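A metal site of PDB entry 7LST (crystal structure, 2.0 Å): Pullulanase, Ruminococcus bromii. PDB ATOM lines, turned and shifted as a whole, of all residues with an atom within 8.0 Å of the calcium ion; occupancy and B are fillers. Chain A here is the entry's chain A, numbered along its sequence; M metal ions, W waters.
OE2 of Glu 268 lies close to N of Gly 289 (3.2 Å). The backbone NH (N) of Asn 167 is in hydrogen-bond range of the side-chain carboxylate (OE1) of Glu 268 (2.9 Å). The side-chain carboxylate of Glu 268 is in salt-bridge range of the guanidinium group of Arg 301, at 3.2 Å. The guanidinium group (NH1) of Arg 301 lies close to the side-chain carboxylate (OD1) of Asp 262, 3.9 Å away. The backbone carbonyl oxygen (O) of Asp 262 is in hydrogen-bond range of the backbone NH (N) of Val 282. OD2 of Asp 262 is in hydrogen-bond range of ND2 of Asn 283 (3.0 Å). N of Asp 262 is in hydrogen-bond range of O of Val 286 (2.7 Å). The side-chain hydroxyl of Ser 290 is in hydrogen-bond range of the side-chain carboxylate of Glu 288, 2.7 Å away.
The calcium ion is bound by OE2 of Glu 268, 2.2 Å away. The calcium ion is bound by O of Phe 263 (2.3 Å). The calcium ion is bound by OD1 of Asp 262. Water W3 is bound to the calcium ion, 2.4 Å away. Water W2 is bound to the calcium ion (2.5 Å). Water W1 is bound to the calcium ion, 2.6 Å away. OE1 of Glu 288 is bound to the calcium ion, 2.6 Å away. The calcium ion has seven donor atoms within binding distance.
Water W1 bridges OD2 of Asp 262 (2.8 Å) and O of Asn 167 (3.2 Å). Water W2 bridges OD1 of Asn 167 and O of Val 266. Water W3 lies within hydrogen-bond range of O of Val 266 (2.5 Å) and OE2 of Glu 288 (2.6 Å).
Four residues have an atom within 4 Å of the calcium ion: Asp 262, Phe 263, Glu 268 and Glu 288. The nearest printed residue that does not touch the calcium ion is Val 266 (4.2 Å).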
ATOM      1  N   THR A 164       4.257 -18.371 -17.191  1.00  0.00           N
ATOM      2  CA  THR A 164       3.454 -19.402 -16.520  1.00  0.00           C
ATOM      3  C   THR A 164       4.179 -19.874 -15.261  1.00  0.00           C
ATOM      4  O   THR A 164       5.375 -19.642 -15.097  1.00  0.00           O
ATOM      5  CB  THR A 164       3.160 -20.597 -17.420  1.00  0.00           C
ATOM      6  OG1 THR A 164       4.392 -21.288 -17.666  1.00  0.00           O
ATOM      7  CG2 THR A 164       2.517 -20.226 -18.743  1.00  0.00           C
ATOM      8  N   GLY A 165       3.419 -20.555 -14.387  1.00  0.00           N
ATOM      9  CA  GLY A 165       3.983 -21.307 -13.272  1.00  0.00           C
ATOM     10  C   GLY A 165       4.538 -22.643 -13.735  1.00  0.00           C
ATOM     11  O   GLY A 165       4.727 -22.846 -14.939  1.00  0.00           O
ATOM     12  N   VAL A 166       4.792 -23.542 -12.785  1.00  0.00           N
ATOM     13  CA  VAL A 166       5.381 -24.858 -13.048  1.00  0.00           C
ATOM     14  C   VAL A 166       4.477 -25.665 -13.999  1.00  0.00           C
ATOM     15  O   VAL A 166       3.278 -25.767 -13.783  1.00  0.00           O
ATOM     16  CB  VAL A 166       5.671 -25.614 -11.739  1.00  0.00           C
ATOM     17  CG1 VAL A 166       4.418 -25.851 -10.889  1.00  0.00           C
ATOM     18  CG2 VAL A 166       6.382 -26.934 -12.004  1.00  0.00           C
ATOM     19  N   ASN A 167       5.084 -26.199 -15.072  1.00  0.00           N
ATOM     20  CA  ASN A 167       4.455 -27.111 -16.040  1.00  0.00           C
ATOM     21  C   ASN A 167       3.367 -26.392 -16.866  1.00  0.00           C
ATOM     22  O   ASN A 167       2.568 -27.046 -17.537  1.00  0.00           O
ATOM     23  CB  ASN A 167       3.933 -28.389 -15.371  1.00  0.00           C
ATOM     24  CG  ASN A 167       5.041 -29.348 -14.988  1.00  0.00           C
ATOM     25  OD1 ASN A 167       6.040 -29.471 -15.701  1.00  0.00           O
ATOM     26  ND2 ASN A 167       4.888 -30.036 -13.870  1.00  0.00           N
ATOM     27  N   GLY A 168       3.375 -25.056 -16.855  1.00  0.00           N
ATOM     28  CA  GLY A 168       2.652 -24.208 -17.821  1.00  0.00           C
ATOM     29  C   GLY A 168       1.133 -24.342 -17.802  1.00  0.00           C
ATOM     30  O   GLY A 168       0.490 -24.133 -18.831  1.00  0.00           O
ATOM     31  N   TYR A 261      11.163 -22.596 -26.056  1.00  0.00           N
ATOM     32  CA  TYR A 261       9.759 -22.363 -25.688  1.00  0.00           C
ATOM     33  C   TYR A 261       9.329 -23.490 -24.741  1.00  0.00           C
ATOM     34  O   TYR A 261       9.988 -24.530 -24.689  1.00  0.00           O
ATOM     35  CB  TYR A 261       8.833 -22.352 -26.916  1.00  0.00           C
ATOM     36  CG  TYR A 261       8.846 -23.652 -27.666  1.00  0.00           C
ATOM     37  CD1 TYR A 261       8.056 -24.722 -27.264  1.00  0.00           C
ATOM     38  CD2 TYR A 261       9.714 -23.852 -28.734  1.00  0.00           C
ATOM     39  CE1 TYR A 261       8.104 -25.937 -27.920  1.00  0.00           C
ATOM     40  CE2 TYR A 261       9.784 -25.069 -29.394  1.00  0.00           C
ATOM     41  CZ  TYR A 261       8.973 -26.108 -28.996  1.00  0.00           C
ATOM     42  OH  TYR A 261       9.027 -27.302 -29.649  1.00  0.00           O
ATOM     43  N   ASP A 262       8.214 -23.280 -24.025  1.00  0.00           N
ATOM     44  CA  ASP A 262       7.745 -24.237 -23.025  1.00  0.00           C
ATOM     45  C   ASP A 262       7.135 -25.464 -23.730  1.00  0.00           C
ATOM     46  O   ASP A 262       6.179 -25.331 -24.492  1.00  0.00           O
ATOM     47  CB  ASP A 262       6.715 -23.581 -22.095  1.00  0.00           C
ATOM     48  CG  ASP A 262       6.310 -24.441 -20.912  1.00  0.00           C
ATOM     49  OD1 ASP A 262       7.201 -25.159 -20.383  1.00  0.00           O
ATOM     50  OD2 ASP A 262       5.127 -24.387 -20.528  1.00  0.00           O
ATOM     51  N   PHE A 263       7.684 -26.651 -23.420  1.00  0.00           N
ATOM     52  CA  PHE A 263       7.203 -27.938 -23.940  1.00  0.00           C
ATOM     53  C   PHE A 263       6.689 -28.802 -22.787  1.00  0.00           C
ATOM     54  O   PHE A 263       6.825 -28.450 -21.609  1.00  0.00           O
ATOM     55  CB  PHE A 263       8.303 -28.620 -24.764  1.00  0.00           C
ATOM     56  CG  PHE A 263       9.653 -28.748 -24.096  1.00  0.00           C
ATOM     57  CD1 PHE A 263       9.921 -29.792 -23.224  1.00  0.00           C
ATOM     58  CD2 PHE A 263      10.671 -27.853 -24.386  1.00  0.00           C
ATOM     59  CE1 PHE A 263      11.168 -29.916 -22.633  1.00  0.00           C
ATOM     60  CE2 PHE A 263      11.918 -27.986 -23.792  1.00  0.00           C
ATOM     61  CZ  PHE A 263      12.164 -29.019 -22.920  1.00  0.00           C
ATOM     62  N   GLN A 264       6.079 -29.946 -23.129  1.00  0.00           N
ATOM     63  CA  GLN A 264       5.306 -30.789 -22.207  1.00  0.00           C
ATOM     64  C   GLN A 264       6.183 -31.849 -21.524  1.00  0.00           C
ATOM     65  O   GLN A 264       5.924 -32.219 -20.387  1.00  0.00           O
ATOM     66  CB  GLN A 264       4.177 -31.486 -22.963  1.00  0.00           C
ATOM     67  CG  GLN A 264       3.252 -32.311 -22.070  1.00  0.00           C
ATOM     68  CD  GLN A 264       3.667 -33.759 -21.942  1.00  0.00           C
ATOM     69  OE1 GLN A 264       4.589 -34.238 -22.603  1.00  0.00           O
ATOM     70  NE2 GLN A 264       2.960 -34.486 -21.085  1.00  0.00           N
ATOM     71  N   SER A 265       7.200 -32.335 -22.242  1.00  0.00           N
ATOM     72  CA  SER A 265       7.769 -33.678 -22.050  1.00  0.00           C
ATOM     73  C   SER A 265       8.802 -33.757 -20.913  1.00  0.00           C
ATOM     74  O   SER A 265       9.331 -34.846 -20.661  1.00  0.00           O
ATOM     75  CB  SER A 265       8.332 -34.187 -23.351  1.00  0.00           C
ATOM     76  OG  SER A 265       9.069 -33.171 -24.006  1.00  0.00           O
ATOM     77  N   VAL A 266       9.087 -32.649 -20.228  1.00  0.00           N
ATOM     78  CA  VAL A 266       9.893 -32.688 -19.004  1.00  0.00           C
ATOM     79  C   VAL A 266       9.021 -32.184 -17.839  1.00  0.00           C
ATOM     80  O   VAL A 266       8.516 -31.061 -17.874  1.00  0.00           O
ATOM     81  CB  VAL A 266      11.207 -31.893 -19.125  1.00  0.00           C
ATOM     82  CG1 VAL A 266      11.861 -31.667 -17.772  1.00  0.00           C
ATOM     83  CG2 VAL A 266      12.182 -32.572 -20.072  1.00  0.00           C
ATOM     84  N   ASN A 267       8.863 -33.032 -16.819  1.00  0.00           N
ATOM     85  CA  ASN A 267       8.190 -32.663 -15.594  1.00  0.00           C
ATOM     86  C   ASN A 267       9.119 -31.724 -14.808  1.00  0.00           C
ATOM     87  O   ASN A 267      10.144 -32.157 -14.281  1.00  0.00           O
ATOM     88  CB  ASN A 267       7.791 -33.879 -14.752  1.00  0.00           C
ATOM     89  CG  ASN A 267       7.062 -33.518 -13.483  1.00  0.00           C
ATOM     90  OD1 ASN A 267       6.630 -32.371 -13.298  1.00  0.00           O
ATOM     91  ND2 ASN A 267       6.911 -34.482 -12.594  1.00  0.00           N
ATOM     92  N   GLU A 268       8.725 -30.452 -14.732  1.00  0.00           N
ATOM     93  CA  GLU A 268       9.566 -29.384 -14.216  1.00  0.00           C
ATOM     94  C   GLU A 268       9.680 -29.478 -12.686  1.00  0.00           C
ATOM     95  O   GLU A 268      10.535 -28.805 -12.100  1.00  0.00           O
ATOM     96  CB  GLU A 268       9.005 -28.021 -14.648  1.00  0.00           C
ATOM     97  CG  GLU A 268       9.030 -27.812 -16.156  1.00  0.00           C
ATOM     98  CD  GLU A 268       8.327 -26.560 -16.634  1.00  0.00           C
ATOM     99  OE1 GLU A 268       7.881 -25.767 -15.781  1.00  0.00           O
ATOM    100  OE2 GLU A 268       8.217 -26.370 -17.870  1.00  0.00           O
ATOM    101  N   ASP A 280       7.423 -30.565 -28.398  1.00  0.00           N
ATOM    102  CA  ASP A 280       6.147 -30.899 -27.764  1.00  0.00           C
ATOM    103  C   ASP A 280       5.544 -29.622 -27.175  1.00  0.00           C
ATOM    104  O   ASP A 280       5.419 -29.491 -25.964  1.00  0.00           O
ATOM    105  CB  ASP A 280       6.335 -31.972 -26.697  1.00  0.00           C
ATOM    106  CG  ASP A 280       7.062 -33.233 -27.168  1.00  0.00           C
ATOM    107  OD1 ASP A 280       6.650 -33.791 -28.217  1.00  0.00           O
ATOM    108  OD2 ASP A 280       8.018 -33.653 -26.478  1.00  0.00           O
ATOM    109  N   VAL A 282       3.581 -26.461 -25.580  1.00  0.00           N
ATOM    110  CA  VAL A 282       2.454 -26.166 -24.696  1.00  0.00           C
ATOM    111  C   VAL A 282       2.193 -24.644 -24.716  1.00  0.00           C
ATOM    112  O   VAL A 282       1.035 -24.227 -24.882  1.00  0.00           O
ATOM    113  CB  VAL A 282       2.716 -26.683 -23.268  1.00  0.00           C
ATOM    114  CG1 VAL A 282       1.514 -26.472 -22.359  1.00  0.00           C
ATOM    115  CG2 VAL A 282       3.108 -28.153 -23.270  1.00  0.00           C
ATOM    116  N   ASN A 283       3.250 -23.850 -24.515  1.00  0.00           N
ATOM    117  CA  ASN A 283       3.167 -22.381 -24.479  1.00  0.00           C
ATOM    118  C   ASN A 283       4.266 -21.798 -25.369  1.00  0.00           C
ATOM    119  O   ASN A 283       5.442 -21.826 -25.014  1.00  0.00           O
ATOM    120  CB  ASN A 283       3.279 -21.841 -23.057  1.00  0.00           C
ATOM    121  CG  ASN A 283       2.168 -22.315 -22.146  1.00  0.00           C
ATOM    122  OD1 ASN A 283       1.019 -21.900 -22.280  1.00  0.00           O
ATOM    123  ND2 ASN A 283       2.501 -23.186 -21.198  1.00  0.00           N
ATOM    124  N   VAL A 286       6.384 -18.571 -23.978  1.00  0.00           N
ATOM    125  CA  VAL A 286       6.920 -18.723 -22.626  1.00  0.00           C
ATOM    126  C   VAL A 286       8.156 -19.599 -22.704  1.00  0.00           C
ATOM    127  O   VAL A 286       8.150 -20.613 -23.391  1.00  0.00           O
ATOM    128  CB  VAL A 286       5.854 -19.311 -21.670  1.00  0.00           C
ATOM    129  CG1 VAL A 286       6.416 -19.602 -20.291  1.00  0.00           C
ATOM    130  CG2 VAL A 286       4.628 -18.418 -21.565  1.00  0.00           C
ATOM    131  N   PRO A 287       9.269 -19.247 -22.007  1.00  0.00           N
ATOM    132  CA  PRO A 287      10.428 -20.136 -21.909  1.00  0.00           C
ATOM    133  C   PRO A 287      10.144 -21.464 -21.204  1.00  0.00           C
ATOM    134  O   PRO A 287       9.255 -21.549 -20.360  1.00  0.00           O
ATOM    135  CB  PRO A 287      11.452 -19.345 -21.083  1.00  0.00           C
ATOM    136  CG  PRO A 287      10.992 -17.902 -21.151  1.00  0.00           C
ATOM    137  CD  PRO A 287       9.491 -17.966 -21.341  1.00  0.00           C
ATOM    138  N   GLU A 288      10.936 -22.498 -21.547  1.00  0.00           N
ATOM    139  CA  GLU A 288      10.887 -23.803 -20.885  1.00  0.00           C
ATOM    140  C   GLU A 288      11.348 -23.648 -19.433  1.00  0.00           C
ATOM    141  O   GLU A 288      12.307 -22.934 -19.153  1.00  0.00           O
ATOM    142  CB  GLU A 288      11.749 -24.818 -21.629  1.00  0.00           C
ATOM    143  CG  GLU A 288      12.040 -26.083 -20.850  1.00  0.00           C
ATOM    144  CD  GLU A 288      10.839 -26.922 -20.448  1.00  0.00           C
ATOM    145  OE1 GLU A 288       9.734 -26.688 -20.994  1.00  0.00           O
ATOM    146  OE2 GLU A 288      10.999 -27.809 -19.583  1.00  0.00           O
ATOM    147  N   GLY A 289      10.646 -24.319 -18.516  1.00  0.00           N
ATOM    148  CA  GLY A 289      10.888 -24.204 -17.081  1.00  0.00           C
ATOM    149  C   GLY A 289      12.095 -24.998 -16.608  1.00  0.00           C
ATOM    150  O   GLY A 289      12.811 -24.551 -15.711  1.00  0.00           O
ATOM    151  N   SER A 290      12.319 -26.171 -17.203  1.00  0.00           N
ATOM    152  CA  SER A 290      13.306 -27.143 -16.725  1.00  0.00           C
ATOM    153  C   SER A 290      14.745 -26.634 -16.899  1.00  0.00           C
ATOM    154  O   SER A 290      15.654 -27.076 -16.181  1.00  0.00           O
ATOM    155  CB  SER A 290      13.122 -28.491 -17.405  1.00  0.00           C
ATOM    156  OG  SER A 290      13.485 -28.424 -18.778  1.00  0.00           O
ATOM    157  N   TYR A 291      14.960 -25.693 -17.831  1.00  0.00           N
ATOM    158  CA  TYR A 291      16.284 -25.100 -18.053  1.00  0.00           C
ATOM    159  C   TYR A 291      16.533 -23.928 -17.087  1.00  0.00           C
ATOM    160  O   TYR A 291      17.622 -23.373 -17.084  1.00  0.00           O
ATOM    161  CB  TYR A 291      16.435 -24.644 -19.510  1.00  0.00           C
ATOM    162  CG  TYR A 291      16.260 -25.741 -20.535  1.00  0.00           C
ATOM    163  CD1 TYR A 291      16.843 -26.993 -20.351  1.00  0.00           C
ATOM    164  CD2 TYR A 291      15.536 -25.533 -21.695  1.00  0.00           C
ATOM    165  CE1 TYR A 291      16.695 -27.993 -21.279  1.00  0.00           C
ATOM    166  CE2 TYR A 291      15.385 -26.528 -22.648  1.00  0.00           C
ATOM    167  CZ  TYR A 291      15.964 -27.773 -22.436  1.00  0.00           C
ATOM    168  OH  TYR A 291      15.813 -28.770 -23.351  1.00  0.00           O
ATOM    169  N   PRO A 295      11.243 -23.058 -11.728  1.00  0.00           N
ATOM    170  CA  PRO A 295      10.094 -22.975 -12.626  1.00  0.00           C
ATOM    171  C   PRO A 295       8.776 -22.551 -11.946  1.00  0.00           C
ATOM    172  O   PRO A 295       7.794 -22.287 -12.644  1.00  0.00           O
ATOM    173  CB  PRO A 295       9.987 -24.420 -13.150  1.00  0.00           C
ATOM    174  CG  PRO A 295      10.483 -25.277 -12.010  1.00  0.00           C
ATOM    175  CD  PRO A 295      11.499 -24.435 -11.266  1.00  0.00           C
ATOM    176  N   ARG A 301      12.557 -17.898 -14.952  1.00  0.00           N
ATOM    177  CA  ARG A 301      12.940 -18.510 -16.232  1.00  0.00           C
ATOM    178  C   ARG A 301      13.105 -17.430 -17.312  1.00  0.00           C
ATOM    179  O   ARG A 301      13.984 -17.557 -18.176  1.00  0.00           O
ATOM    180  CB  ARG A 301      11.933 -19.578 -16.649  1.00  0.00           C
ATOM    181  CG  ARG A 301      10.561 -19.062 -17.060  1.00  0.00           C
ATOM    182  CD  ARG A 301       9.658 -20.182 -17.543  1.00  0.00           C
ATOM    183  NE  ARG A 301       9.095 -20.966 -16.449  1.00  0.00           N
ATOM    184  CZ  ARG A 301       8.210 -21.938 -16.598  1.00  0.00           C
ATOM    185  NH1 ARG A 301       7.785 -22.278 -17.803  1.00  0.00           N
ATOM    186  NH2 ARG A 301       7.743 -22.578 -15.534  1.00  0.00           N
HETATM  187 CA    CA M   1       7.580 -27.394 -19.749  1.00  0.00          CA
HETATM  188  O   HOH W   1       5.066 -26.991 -19.577  1.00  0.00           O
HETATM  189  O   HOH W   2       6.531 -29.099 -18.200  1.00  0.00           O
HETATM  190  O   HOH W   3       8.928 -29.399 -19.748  1.00  0.00           O
